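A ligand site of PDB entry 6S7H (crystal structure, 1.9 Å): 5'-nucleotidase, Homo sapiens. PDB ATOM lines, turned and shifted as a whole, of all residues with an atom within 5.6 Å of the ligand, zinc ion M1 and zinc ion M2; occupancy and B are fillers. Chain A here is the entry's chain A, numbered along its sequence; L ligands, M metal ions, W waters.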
ATOM      1  N   ASP A  11     -14.759  -6.473  21.199  1.00  0.00           N
ATOM      2  CA  ASP A  11     -15.910  -5.596  21.339  1.00  0.00           C
ATOM      3  C   ASP A  11     -16.175  -4.751  20.073  1.00  0.00           C
ATOM      4  O   ASP A  11     -16.439  -3.556  20.148  1.00  0.00           O
ATOM      5  CB  ASP A  11     -15.754  -4.748  22.632  1.00  0.00           C
ATOM      6  CG  ASP A  11     -15.635  -5.662  23.844  1.00  0.00           C
ATOM      7  OD1 ASP A  11     -14.519  -6.142  24.111  1.00  0.00           O
ATOM      8  OD2 ASP A  11     -16.666  -5.926  24.494  1.00  0.00           O
ATOM      9  N   HIS A  13     -18.698  -4.965  18.112  1.00  0.00           N
ATOM     10  CA  HIS A  13     -20.080  -4.517  18.212  1.00  0.00           C
ATOM     11  C   HIS A  13     -20.673  -3.953  16.898  1.00  0.00           C
ATOM     12  O   HIS A  13     -21.178  -2.822  16.859  1.00  0.00           O
ATOM     13  CB  HIS A  13     -20.256  -3.515  19.410  1.00  0.00           C
ATOM     14  CG  HIS A  13     -20.168  -4.212  20.712  1.00  0.00           C
ATOM     15  ND1 HIS A  13     -20.969  -5.298  20.989  1.00  0.00           N
ATOM     16  CD2 HIS A  13     -19.264  -4.056  21.711  1.00  0.00           C
ATOM     17  CE1 HIS A  13     -20.580  -5.741  22.178  1.00  0.00           C
ATOM     18  NE2 HIS A  13     -19.570  -5.006  22.668  1.00  0.00           N
ATOM     19  N   ASP A  60     -17.650 -10.324  21.541  1.00  0.00           N
ATOM     20  CA  ASP A  60     -18.544  -9.188  21.398  1.00  0.00           C
ATOM     21  C   ASP A  60     -18.481  -8.520  20.011  1.00  0.00           C
ATOM     22  O   ASP A  60     -18.419  -7.289  19.874  1.00  0.00           O
ATOM     23  CB  ASP A  60     -18.315  -8.192  22.514  1.00  0.00           C
ATOM     24  CG  ASP A  60     -19.095  -8.443  23.783  1.00  0.00           C
ATOM     25  OD1 ASP A  60     -19.656  -9.569  23.941  1.00  0.00           O
ATOM     26  OD2 ASP A  60     -19.140  -7.507  24.645  1.00  0.00           O
ATOM     27  N   GLY A  91     -17.972 -14.150  23.412  1.00  0.00           N
ATOM     28  CA  GLY A  91     -18.261 -13.054  24.328  1.00  0.00           C
ATOM     29  C   GLY A  91     -19.679 -13.160  24.821  1.00  0.00           C
ATOM     30  O   GLY A  91     -20.451 -13.983  24.338  1.00  0.00           O
ATOM     31  N   ASN A  92     -20.039 -12.327  25.804  1.00  0.00           N
ATOM     32  CA  ASN A  92     -21.409 -12.326  26.336  1.00  0.00           C
ATOM     33  C   ASN A  92     -22.470 -11.920  25.301  1.00  0.00           C
ATOM     34  O   ASN A  92     -23.498 -12.586  25.230  1.00  0.00           O
ATOM     35  CB  ASN A  92     -21.543 -11.466  27.603  1.00  0.00           C
ATOM     36  CG  ASN A  92     -20.990 -10.083  27.534  1.00  0.00           C
ATOM     37  OD1 ASN A  92     -19.754  -9.886  27.406  1.00  0.00           O
ATOM     38  ND2 ASN A  92     -21.863  -9.089  27.600  1.00  0.00           N
ATOM     39  N   HIS A  93     -22.192 -10.934  24.430  1.00  0.00           N
ATOM     40  CA  HIS A  93     -23.192 -10.503  23.445  1.00  0.00           C
ATOM     41  C   HIS A  93     -23.397 -11.529  22.345  1.00  0.00           C
ATOM     42  O   HIS A  93     -24.422 -11.471  21.687  1.00  0.00           O
ATOM     43  CB  HIS A  93     -22.931  -9.088  22.924  1.00  0.00           C
ATOM     44  CG  HIS A  93     -23.203  -8.051  23.967  1.00  0.00           C
ATOM     45  ND1 HIS A  93     -24.464  -7.580  24.190  1.00  0.00           N
ATOM     46  CD2 HIS A  93     -22.373  -7.500  24.879  1.00  0.00           C
ATOM     47  CE1 HIS A  93     -24.376  -6.731  25.205  1.00  0.00           C
ATOM     48  NE2 HIS A  93     -23.122  -6.635  25.639  1.00  0.00           N
ATOM     49  N   ASP A  96     -26.890 -13.007  23.118  1.00  0.00           N
ATOM     50  CA  ASP A  96     -28.061 -12.115  23.182  1.00  0.00           C
ATOM     51  C   ASP A  96     -29.321 -12.637  22.500  1.00  0.00           C
ATOM     52  O   ASP A  96     -30.421 -12.344  22.967  1.00  0.00           O
ATOM     53  CB  ASP A  96     -27.713 -10.736  22.609  1.00  0.00           C
ATOM     54  CG  ASP A  96     -26.849  -9.842  23.495  1.00  0.00           C
ATOM     55  OD1 ASP A  96     -26.400 -10.304  24.572  1.00  0.00           O
ATOM     56  OD2 ASP A  96     -26.573  -8.713  23.087  1.00  0.00           O
ATOM     57  N   PHE A 158     -26.030 -13.679  33.732  1.00  0.00           N
ATOM     58  CA  PHE A 158     -26.633 -12.423  34.203  1.00  0.00           C
ATOM     59  C   PHE A 158     -26.542 -11.281  33.172  1.00  0.00           C
ATOM     60  O   PHE A 158     -27.288 -10.306  33.304  1.00  0.00           O
ATOM     61  CB  PHE A 158     -25.937 -11.952  35.490  1.00  0.00           C
ATOM     62  CG  PHE A 158     -25.967 -12.963  36.607  1.00  0.00           C
ATOM     63  CD1 PHE A 158     -27.159 -13.280  37.233  1.00  0.00           C
ATOM     64  CD2 PHE A 158     -24.804 -13.603  37.020  1.00  0.00           C
ATOM     65  CE1 PHE A 158     -27.189 -14.231  38.259  1.00  0.00           C
ATOM     66  CE2 PHE A 158     -24.837 -14.532  38.055  1.00  0.00           C
ATOM     67  CZ  PHE A 158     -26.029 -14.851  38.657  1.00  0.00           C
ATOM     68  N   LEU A 159     -25.599 -11.344  32.207  1.00  0.00           N
ATOM     69  CA  LEU A 159     -25.386 -10.300  31.204  1.00  0.00           C
ATOM     70  C   LEU A 159     -26.164 -10.532  29.912  1.00  0.00           C
ATOM     71  O   LEU A 159     -26.349  -9.577  29.134  1.00  0.00           O
ATOM     72  CB  LEU A 159     -23.906 -10.208  30.846  1.00  0.00           C
ATOM     73  CG  LEU A 159     -22.934  -9.991  31.994  1.00  0.00           C
ATOM     74  CD1 LEU A 159     -21.511 -10.190  31.538  1.00  0.00           C
ATOM     75  CD2 LEU A 159     -23.087  -8.616  32.606  1.00  0.00           C
ATOM     76  N   SER A 160     -26.557 -11.775  29.634  1.00  0.00           N
ATOM     77  CA  SER A 160     -27.184 -12.131  28.356  1.00  0.00           C
ATOM     78  C   SER A 160     -28.251 -13.207  28.567  1.00  0.00           C
ATOM     79  O   SER A 160     -28.752 -13.350  29.689  1.00  0.00           O
ATOM     80  CB  SER A 160     -26.088 -12.642  27.412  1.00  0.00           C
ATOM     81  OG  SER A 160     -26.524 -12.649  26.061  1.00  0.00           O
ATOM     82  N   ASN A 161     -28.616 -13.918  27.485  1.00  0.00           N
ATOM     83  CA  ASN A 161     -29.580 -15.020  27.532  1.00  0.00           C
ATOM     84  C   ASN A 161     -28.942 -16.347  27.030  1.00  0.00           C
ATOM     85  O   ASN A 161     -29.393 -16.922  26.048  1.00  0.00           O
ATOM     86  CB  ASN A 161     -30.855 -14.640  26.741  1.00  0.00           C
ATOM     87  CG  ASN A 161     -32.073 -15.474  27.107  1.00  0.00           C
ATOM     88  OD1 ASN A 161     -32.065 -16.237  28.083  1.00  0.00           O
ATOM     89  ND2 ASN A 161     -33.112 -15.412  26.283  1.00  0.00           N
ATOM     90  N   HIS A 195     -13.080 -13.371  26.878  1.00  0.00           N
ATOM     91  CA  HIS A 195     -13.990 -12.254  27.088  1.00  0.00           C
ATOM     92  C   HIS A 195     -14.512 -12.121  28.514  1.00  0.00           C
ATOM     93  O   HIS A 195     -15.689 -12.412  28.774  1.00  0.00           O
ATOM     94  CB  HIS A 195     -15.145 -12.391  26.071  1.00  0.00           C
ATOM     95  CG  HIS A 195     -15.887 -11.118  25.887  1.00  0.00           C
ATOM     96  ND1 HIS A 195     -15.427 -10.133  25.038  1.00  0.00           N
ATOM     97  CD2 HIS A 195     -16.943 -10.651  26.565  1.00  0.00           C
ATOM     98  CE1 HIS A 195     -16.272  -9.131  25.182  1.00  0.00           C
ATOM     99  NE2 HIS A 195     -17.182  -9.395  26.097  1.00  0.00           N
ATOM    100  N   HIS A 218     -14.129  -7.182  26.649  1.00  0.00           N
ATOM    101  CA  HIS A 218     -15.245  -6.969  27.559  1.00  0.00           C
ATOM    102  C   HIS A 218     -15.200  -5.611  28.324  1.00  0.00           C
ATOM    103  O   HIS A 218     -16.253  -5.056  28.579  1.00  0.00           O
ATOM    104  CB  HIS A 218     -15.419  -8.140  28.531  1.00  0.00           C
ATOM    105  CG  HIS A 218     -16.662  -8.078  29.345  1.00  0.00           C
ATOM    106  ND1 HIS A 218     -17.911  -8.143  28.762  1.00  0.00           N
ATOM    107  CD2 HIS A 218     -16.800  -7.935  30.675  1.00  0.00           C
ATOM    108  CE1 HIS A 218     -18.765  -8.052  29.770  1.00  0.00           C
ATOM    109  NE2 HIS A 218     -18.138  -7.906  30.940  1.00  0.00           N
ATOM    110  N   SER A 219     -14.026  -5.149  28.782  1.00  0.00           N
ATOM    111  CA  SER A 219     -13.924  -3.886  29.520  1.00  0.00           C
ATOM    112  C   SER A 219     -13.526  -2.684  28.596  1.00  0.00           C
ATOM    113  O   SER A 219     -13.431  -1.566  29.076  1.00  0.00           O
ATOM    114  CB  SER A 219     -12.969  -4.044  30.701  1.00  0.00           C
ATOM    115  OG  SER A 219     -11.778  -4.695  30.312  1.00  0.00           O
ATOM    116  N   ASN A 220     -13.410  -2.902  27.275  1.00  0.00           N
ATOM    117  CA  ASN A 220     -13.057  -1.884  26.281  1.00  0.00           C
ATOM    118  C   ASN A 220     -11.777  -1.158  26.684  1.00  0.00           C
ATOM    119  O   ASN A 220     -11.675   0.039  26.515  1.00  0.00           O
ATOM    120  CB  ASN A 220     -14.208  -0.892  26.093  1.00  0.00           C
ATOM    121  CG  ASN A 220     -15.523  -1.575  25.840  1.00  0.00           C
ATOM    122  OD1 ASN A 220     -15.623  -2.581  25.122  1.00  0.00           O
ATOM    123  ND2 ASN A 220     -16.581  -1.074  26.448  1.00  0.00           N
ATOM    124  N   ARG A 329     -21.310   7.269  31.757  1.00  0.00           N
ATOM    125  CA  ARG A 329     -20.987   6.423  32.897  1.00  0.00           C
ATOM    126  C   ARG A 329     -20.310   7.231  34.023  1.00  0.00           C
ATOM    127  O   ARG A 329     -19.931   6.658  35.015  1.00  0.00           O
ATOM    128  CB  ARG A 329     -20.077   5.256  32.475  1.00  0.00           C
ATOM    129  CG  ARG A 329     -20.699   4.407  31.396  1.00  0.00           C
ATOM    130  CD  ARG A 329     -19.905   3.173  31.110  1.00  0.00           C
ATOM    131  NE  ARG A 329     -20.468   2.454  29.957  1.00  0.00           N
ATOM    132  CZ  ARG A 329     -20.290   1.161  29.705  1.00  0.00           C
ATOM    133  NH1 ARG A 329     -19.549   0.416  30.514  1.00  0.00           N
ATOM    134  NH2 ARG A 329     -20.847   0.613  28.627  1.00  0.00           N
ATOM    135  N   ASN A 365     -29.667   3.128  33.257  1.00  0.00           N
ATOM    136  CA  ASN A 365     -28.231   2.787  33.340  1.00  0.00           C
ATOM    137  C   ASN A 365     -27.507   3.402  32.153  1.00  0.00           C
ATOM    138  O   ASN A 365     -27.901   3.161  30.995  1.00  0.00           O
ATOM    139  CB  ASN A 365     -27.998   1.261  33.372  1.00  0.00           C
ATOM    140  CG  ASN A 365     -28.754   0.477  32.307  1.00  0.00           C
ATOM    141  OD1 ASN A 365     -29.979   0.541  32.210  1.00  0.00           O
ATOM    142  ND2 ASN A 365     -28.057  -0.263  31.463  1.00  0.00           N
ATOM    143  N   GLY A 366     -26.464   4.206  32.415  1.00  0.00           N
ATOM    144  CA  GLY A 366     -25.674   4.852  31.373  1.00  0.00           C
ATOM    145  C   GLY A 366     -25.028   3.894  30.385  1.00  0.00           C
ATOM    146  O   GLY A 366     -24.910   4.216  29.198  1.00  0.00           O
ATOM    147  N   GLY A 367     -24.686   2.686  30.857  1.00  0.00           N
ATOM    148  CA  GLY A 367     -24.133   1.658  30.001  1.00  0.00           C
ATOM    149  C   GLY A 367     -25.097   1.128  28.941  1.00  0.00           C
ATOM    150  O   GLY A 367     -24.665   0.526  27.960  1.00  0.00           O
ATOM    151  N   GLY A 368     -26.406   1.327  29.142  1.00  0.00           N
ATOM    152  CA  GLY A 368     -27.417   0.974  28.156  1.00  0.00           C
ATOM    153  C   GLY A 368     -27.445   1.905  26.951  1.00  0.00           C
ATOM    154  O   GLY A 368     -28.037   1.568  25.931  1.00  0.00           O
ATOM    155  N   ARG A 370     -25.648   3.083  24.024  1.00  0.00           N
ATOM    156  CA  ARG A 370     -24.529   2.391  23.372  1.00  0.00           C
ATOM    157  C   ARG A 370     -23.776   3.188  22.317  1.00  0.00           C
ATOM    158  O   ARG A 370     -22.737   2.701  21.831  1.00  0.00           O
ATOM    159  CB  ARG A 370     -25.003   1.053  22.764  1.00  0.00           C
ATOM    160  CG  ARG A 370     -25.586   0.076  23.771  1.00  0.00           C
ATOM    161  CD  ARG A 370     -24.574  -0.494  24.782  1.00  0.00           C
ATOM    162  NE  ARG A 370     -23.705  -1.529  24.219  1.00  0.00           N
ATOM    163  CZ  ARG A 370     -22.907  -2.344  24.919  1.00  0.00           C
ATOM    164  NH1 ARG A 370     -22.155  -3.247  24.304  1.00  0.00           N
ATOM    165  NH2 ARG A 370     -22.861  -2.249  26.246  1.00  0.00           N
ATOM    166  N   PHE A 392     -30.678  -3.211  21.926  1.00  0.00           N
ATOM    167  CA  PHE A 392     -31.099  -4.429  22.609  1.00  0.00           C
ATOM    168  C   PHE A 392     -32.551  -4.857  22.485  1.00  0.00           C
ATOM    169  O   PHE A 392     -32.857  -5.976  22.900  1.00  0.00           O
ATOM    170  CB  PHE A 392     -30.780  -4.312  24.113  1.00  0.00           C
ATOM    171  CG  PHE A 392     -29.320  -4.028  24.392  1.00  0.00           C
ATOM    172  CD1 PHE A 392     -28.322  -4.859  23.886  1.00  0.00           C
ATOM    173  CD2 PHE A 392     -28.944  -2.929  25.118  1.00  0.00           C
ATOM    174  CE1 PHE A 392     -26.984  -4.547  24.094  1.00  0.00           C
ATOM    175  CE2 PHE A 392     -27.599  -2.625  25.323  1.00  0.00           C
ATOM    176  CZ  PHE A 392     -26.629  -3.464  24.838  1.00  0.00           C
ATOM    177  N   SER A 420     -15.684   3.172  34.859  1.00  0.00           N
ATOM    178  CA  SER A 420     -16.428   3.187  33.579  1.00  0.00           C
ATOM    179  C   SER A 420     -17.460   2.027  33.501  1.00  0.00           C
ATOM    180  O   SER A 420     -17.582   1.339  32.493  1.00  0.00           O
ATOM    181  CB  SER A 420     -15.473   3.174  32.381  1.00  0.00           C
ATOM    182  OG  SER A 420     -16.081   3.597  31.163  1.00  0.00           O
ATOM    183  N   THR A 421     -18.169   1.829  34.595  1.00  0.00           N
ATOM    184  CA  THR A 421     -19.160   0.751  34.692  1.00  0.00           C
ATOM    185  C   THR A 421     -20.521   1.321  34.336  1.00  0.00           C
ATOM    186  O   THR A 421     -20.821   2.504  34.576  1.00  0.00           O
ATOM    187  CB  THR A 421     -19.067   0.033  36.046  1.00  0.00           C
ATOM    188  OG1 THR A 421     -19.284   0.986  37.098  1.00  0.00           O
ATOM    189  CG2 THR A 421     -17.763  -0.695  36.221  1.00  0.00           C
ATOM    190  N   GLY A 422     -21.325   0.467  33.721  1.00  0.00           N
ATOM    191  CA  GLY A 422     -22.608   0.838  33.186  1.00  0.00           C
ATOM    192  C   GLY A 422     -23.717   1.189  34.143  1.00  0.00           C
ATOM    193  O   GLY A 422     -24.697   1.748  33.698  1.00  0.00           O
ATOM    194  N   GLU A 423     -23.582   0.863  35.454  1.00  0.00           N
ATOM    195  CA  GLU A 423     -24.618   1.132  36.456  1.00  0.00           C
ATOM    196  C   GLU A 423     -24.892   2.613  36.776  1.00  0.00           C
ATOM    197  O   GLU A 423     -25.865   2.898  37.444  1.00  0.00           O
ATOM    198  CB  GLU A 423     -24.370   0.393  37.782  1.00  0.00           C
ATOM    199  CG  GLU A 423     -23.190   0.879  38.616  1.00  0.00           C
ATOM    200  CD  GLU A 423     -21.887   0.163  38.353  1.00  0.00           C
ATOM    201  OE1 GLU A 423     -20.951   0.365  39.168  1.00  0.00           O
ATOM    202  OE2 GLU A 423     -21.781  -0.557  37.343  1.00  0.00           O
ATOM    203  N   PRO A 473     -35.654   0.908  32.297  1.00  0.00           N
ATOM    204  CA  PRO A 473     -35.555  -0.268  31.410  1.00  0.00           C
ATOM    205  C   PRO A 473     -35.900  -1.552  32.144  1.00  0.00           C
ATOM    206  O   PRO A 473     -35.589  -1.647  33.334  1.00  0.00           O
ATOM    207  CB  PRO A 473     -34.074  -0.256  30.997  1.00  0.00           C
ATOM    208  CG  PRO A 473     -33.611   1.120  31.253  1.00  0.00           C
ATOM    209  CD  PRO A 473     -34.336   1.538  32.474  1.00  0.00           C
ATOM    210  N   PHE A 475     -34.293  -4.175  31.898  1.00  0.00           N
ATOM    211  CA  PHE A 475     -32.965  -4.576  32.309  1.00  0.00           C
ATOM    212  C   PHE A 475     -32.737  -4.234  33.782  1.00  0.00           C
ATOM    213  O   PHE A 475     -32.283  -5.088  34.532  1.00  0.00           O
ATOM    214  CB  PHE A 475     -31.924  -3.912  31.399  1.00  0.00           C
ATOM    215  CG  PHE A 475     -30.502  -4.181  31.811  1.00  0.00           C
ATOM    216  CD1 PHE A 475     -29.918  -5.416  31.572  1.00  0.00           C
ATOM    217  CD2 PHE A 475     -29.766  -3.235  32.499  1.00  0.00           C
ATOM    218  CE1 PHE A 475     -28.649  -5.710  32.046  1.00  0.00           C
ATOM    219  CE2 PHE A 475     -28.478  -3.512  32.918  1.00  0.00           C
ATOM    220  CZ  PHE A 475     -27.930  -4.739  32.678  1.00  0.00           C
ATOM    221  N   ASP A 481     -27.184  -4.996  36.099  1.00  0.00           N
ATOM    222  CA  ASP A 481     -26.147  -4.076  36.584  1.00  0.00           C
ATOM    223  C   ASP A 481     -26.022  -4.055  38.112  1.00  0.00           C
ATOM    224  O   ASP A 481     -25.572  -3.055  38.662  1.00  0.00           O
ATOM    225  CB  ASP A 481     -26.352  -2.649  35.998  1.00  0.00           C
ATOM    226  CG  ASP A 481     -25.534  -2.343  34.764  1.00  0.00           C
ATOM    227  OD1 ASP A 481     -24.654  -3.159  34.410  1.00  0.00           O
ATOM    228  OD2 ASP A 481     -25.764  -1.286  34.153  1.00  0.00           O
HETATM  229  N1  LIG L   1     -29.712  -3.966  28.363  1.00  0.00           N
HETATM  230  N2  LIG L   1     -28.012  -2.454  29.155  1.00  0.00           N
HETATM  231  C1  LIG L   1     -27.135  -3.417  28.842  1.00  0.00           C
HETATM  232  C2  LIG L   1     -27.416  -4.621  28.227  1.00  0.00           C
HETATM  233  C3  LIG L   1     -28.794  -4.869  27.956  1.00  0.00           C
HETATM  234  C4  LIG L   1     -25.308  -4.532  28.429  1.00  0.00           C
HETATM  235  C5  LIG L   1     -30.764  -6.176  27.199  1.00  0.00           C
HETATM  236  C6  LIG L   1     -28.575  -7.258  27.098  1.00  0.00           C
HETATM  237  C7  LIG L   1     -30.567 -10.655  28.827  1.00  0.00           C
HETATM  238  C8  LIG L   1     -29.716  -9.496  26.901  1.00  0.00           C
HETATM  239  C9  LIG L   1     -29.379  -8.581  29.084  1.00  0.00           C
HETATM  240  P1  LIG L   1     -20.411  -5.471  27.112  1.00  0.00           P
HETATM  241  O1  LIG L   1     -20.230  -6.955  27.257  1.00  0.00           O
HETATM  242  O2  LIG L   1     -21.871  -5.099  27.449  1.00  0.00           O
HETATM  243  O3  LIG L   1     -20.236  -4.950  25.672  1.00  0.00           O
HETATM  244  P2  LIG L   1     -19.492  -2.732  28.233  1.00  0.00           P
HETATM  245  O4  LIG L   1     -18.550  -2.013  29.172  1.00  0.00           O
HETATM  246  O5  LIG L   1     -19.224  -2.132  26.832  1.00  0.00           O
HETATM  247  C10 LIG L   1     -19.315  -4.515  28.158  1.00  0.00           C
HETATM  248  O6  LIG L   1     -20.995  -2.416  28.589  1.00  0.00           O
HETATM  249  C11 LIG L   1     -21.552  -2.908  29.827  1.00  0.00           C
HETATM  250  C12 LIG L   1     -22.810  -2.175  30.216  1.00  0.00           C
HETATM  251  O7  LIG L   1     -23.752  -2.219  29.128  1.00  0.00           O
HETATM  252  C13 LIG L   1     -23.531  -2.842  31.389  1.00  0.00           C
HETATM  253  O8  LIG L   1     -22.925  -2.467  32.615  1.00  0.00           O
HETATM  254  C14 LIG L   1     -24.973  -2.411  31.174  1.00  0.00           C
HETATM  255  O9  LIG L   1     -25.242  -1.145  31.722  1.00  0.00           O
HETATM  256  C15 LIG L   1     -25.062  -2.302  29.651  1.00  0.00           C
HETATM  257  N3  LIG L   1     -25.781  -3.380  28.985  1.00  0.00           N
HETATM  258  N4  LIG L   1     -26.247  -5.304  27.949  1.00  0.00           N
HETATM  259  N5  LIG L   1     -29.319  -6.044  27.441  1.00  0.00           N
HETATM  260  C16 LIG L   1     -29.251  -2.833  28.858  1.00  0.00           C
HETATM  261  C17 LIG L   1     -30.404 -10.568  27.457  1.00  0.00           C
HETATM  262  C18 LIG L   1     -29.205  -8.493  27.707  1.00  0.00           C
HETATM  263  C19 LIG L   1     -30.061  -9.659  29.638  1.00  0.00           C
HETATM  264 CL1  LIG L   1     -30.468  -1.624  29.184  1.00  0.00          CL
HETATM  265 ZN    ZN M   1     -18.649  -5.410  24.372  1.00  0.00          ZN
HETATM  266 ZN    ZN M   2     -18.779  -8.233  26.824  1.00  0.00          ZN
HETATM  267  O   HOH W   1     -17.798  -2.636  31.712  1.00  0.00           O
HETATM  268  O   HOH W   2     -24.736  -6.274  31.220  1.00  0.00           O
HETATM  269  O   HOH W   3     -17.724  -5.151  31.175  1.00  0.00           O
HETATM  270  O   HOH W   4     -16.224  -0.716  29.721  1.00  0.00           O
HETATM  271  O   HOH W   5     -18.110  -3.607  24.803  1.00  0.00           O
HETATM  272  O   HOH W   6     -20.412  -2.275  33.429  1.00  0.00           O
HETATM  273  O   HOH W   7     -20.251  -0.106  25.369  1.00  0.00           O
HETATM  274  O   HOH W   8     -22.404  -6.650  29.703  1.00  0.00           O
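A ring nitrogen (NE2) of His 93 lies within hydrogen-bond range of an oxygen (O2) of the ligand, at 2.7 Å.
An oxygen (O9) of the ligand lies within hydrogen-bond range of the side-chain carboxylate of Asp 481 (2.5 Å).
The guanidinium group (NH1) of Arg 329 is in salt-bridge range of an oxygen (O4) of the ligand.
The guanidinium group (NH2) of Arg 370 is in salt-bridge range of an oxygen (O2) of the ligand (3.2 Å).
O5 of the ligand is in hydrogen-bond range of ND2 of Asn 220.
The side-chain amide nitrogen (ND2) of Asn 365 lies within hydrogen-bond range of an oxygen (O9) of the ligand, 3.0 Å away.
The backbone NH of His 218 lies within hydrogen-bond range of the side-chain carboxylate of Asp 11 (2.8 Å).
NH1 of Arg 329 sits at hydrogen-bond distance from O of Ser 420, at 2.9 Å.
The side-chain hydroxyl (OG) of Ser 160 lies within hydrogen-bond range of the side-chain carboxylate (OD1) of Asp 96 (2.8 Å).
OD1 of Asp 60 is in hydrogen-bond range of N of His 93, 2.9 Å away.
The backbone carbonyl oxygen (O) of Asn 92 is in hydrogen-bond range of the side-chain hydroxyl (OG) of Ser 160 (3.1 Å).
The side-chain carboxylate (OD2) of Asp 481 lies within hydrogen-bond range of the backbone NH (N) of Glu 423, at 3.3 Å.
A ring nitrogen (NE2) of His 93 sits close to the side-chain amide nitrogen (ND2) of Asn 92 (3.4 Å).
OD2 of Asp 96 lies within hydrogen-bond range of ND1 of His 93, at 2.6 Å.
The backbone carbonyl oxygen of Gly 367 sits close to an oxygen (O7) of the ligand (3.1 Å).
Leu 159 touches the ligand (O to C9, 3.2 Å).
Ser 160 touches the ligand (O to C7, 3.4 Å).
Asn 161 touches the ligand (N to C17, 3.8 Å).
Gly 368 touches the ligand (CA to N2, 3.6 Å).
Phe 392 touches the ligand.
CA of Gly 422 touches O8 of the ligand (3.4 Å).
Phe 475 touches the ligand (CG to C16, 3.5 Å).
19 residues have an atom within 4 Å of the ligand: Asp 11, His 13, Asp 60, Asn 92, His 93, Leu 159, Ser 160, Asn 161, His 218, Asn 220, Arg 329, Asn 365, Gly 367, Gly 368, Arg 370, Phe 392, Gly 422, Phe 475 and Asp 481.
The nearest printed residue that does not touch zinc ion M1 is Arg 370 (4.1 Å).
Five residues have an atom within 4 Å of zinc ion M2: Asp 11, Asp 60, Asn 92, His 195 and His 218.
Zinc ion M1 is bound by water W5 (1.9 Å), a ring nitrogen (NE2) of His 13 (2.0 Å), the side-chain carboxylate of Asp 11 (2.1 Å), an oxygen (O3) of the ligand (2.1 Å) and the side-chain carboxylate of Asp 60 (2.2 Å).
Zinc ion M1 has five donor atoms within binding distance.
Zinc ion M2 is bound by an oxygen (O1) of the ligand (2.0 Å), the side-chain amide oxygen of Asn 92 (2.0 Å), a ring nitrogen (NE2) of His 195 (2.1 Å), a ring nitrogen (ND1) of His 218 (2.1 Å) and the side-chain carboxylate of Asp 60 (2.3 Å).
Water W5 bridges OD1 of Asn 220 (2.7 Å) and O5 of the ligand (2.7 Å).
Water W6 bridges O8 of the ligand (2.6 Å) and N of Gly 422 (2.9 Å).
Water W7 lies within hydrogen-bond range of O5 of the ligand, NH2 of Arg 329 and NH2 of Arg 370.
Water W4 lies within hydrogen-bond range of O4 of the ligand (2.7 Å), O of Ser 219 (3.0 Å) and ND2 of Asn 220 (3.3 Å).
Water W8 lies within hydrogen-bond range of O2 of the ligand (2.8 Å) and ND2 of Asn 92 (3.3 Å).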
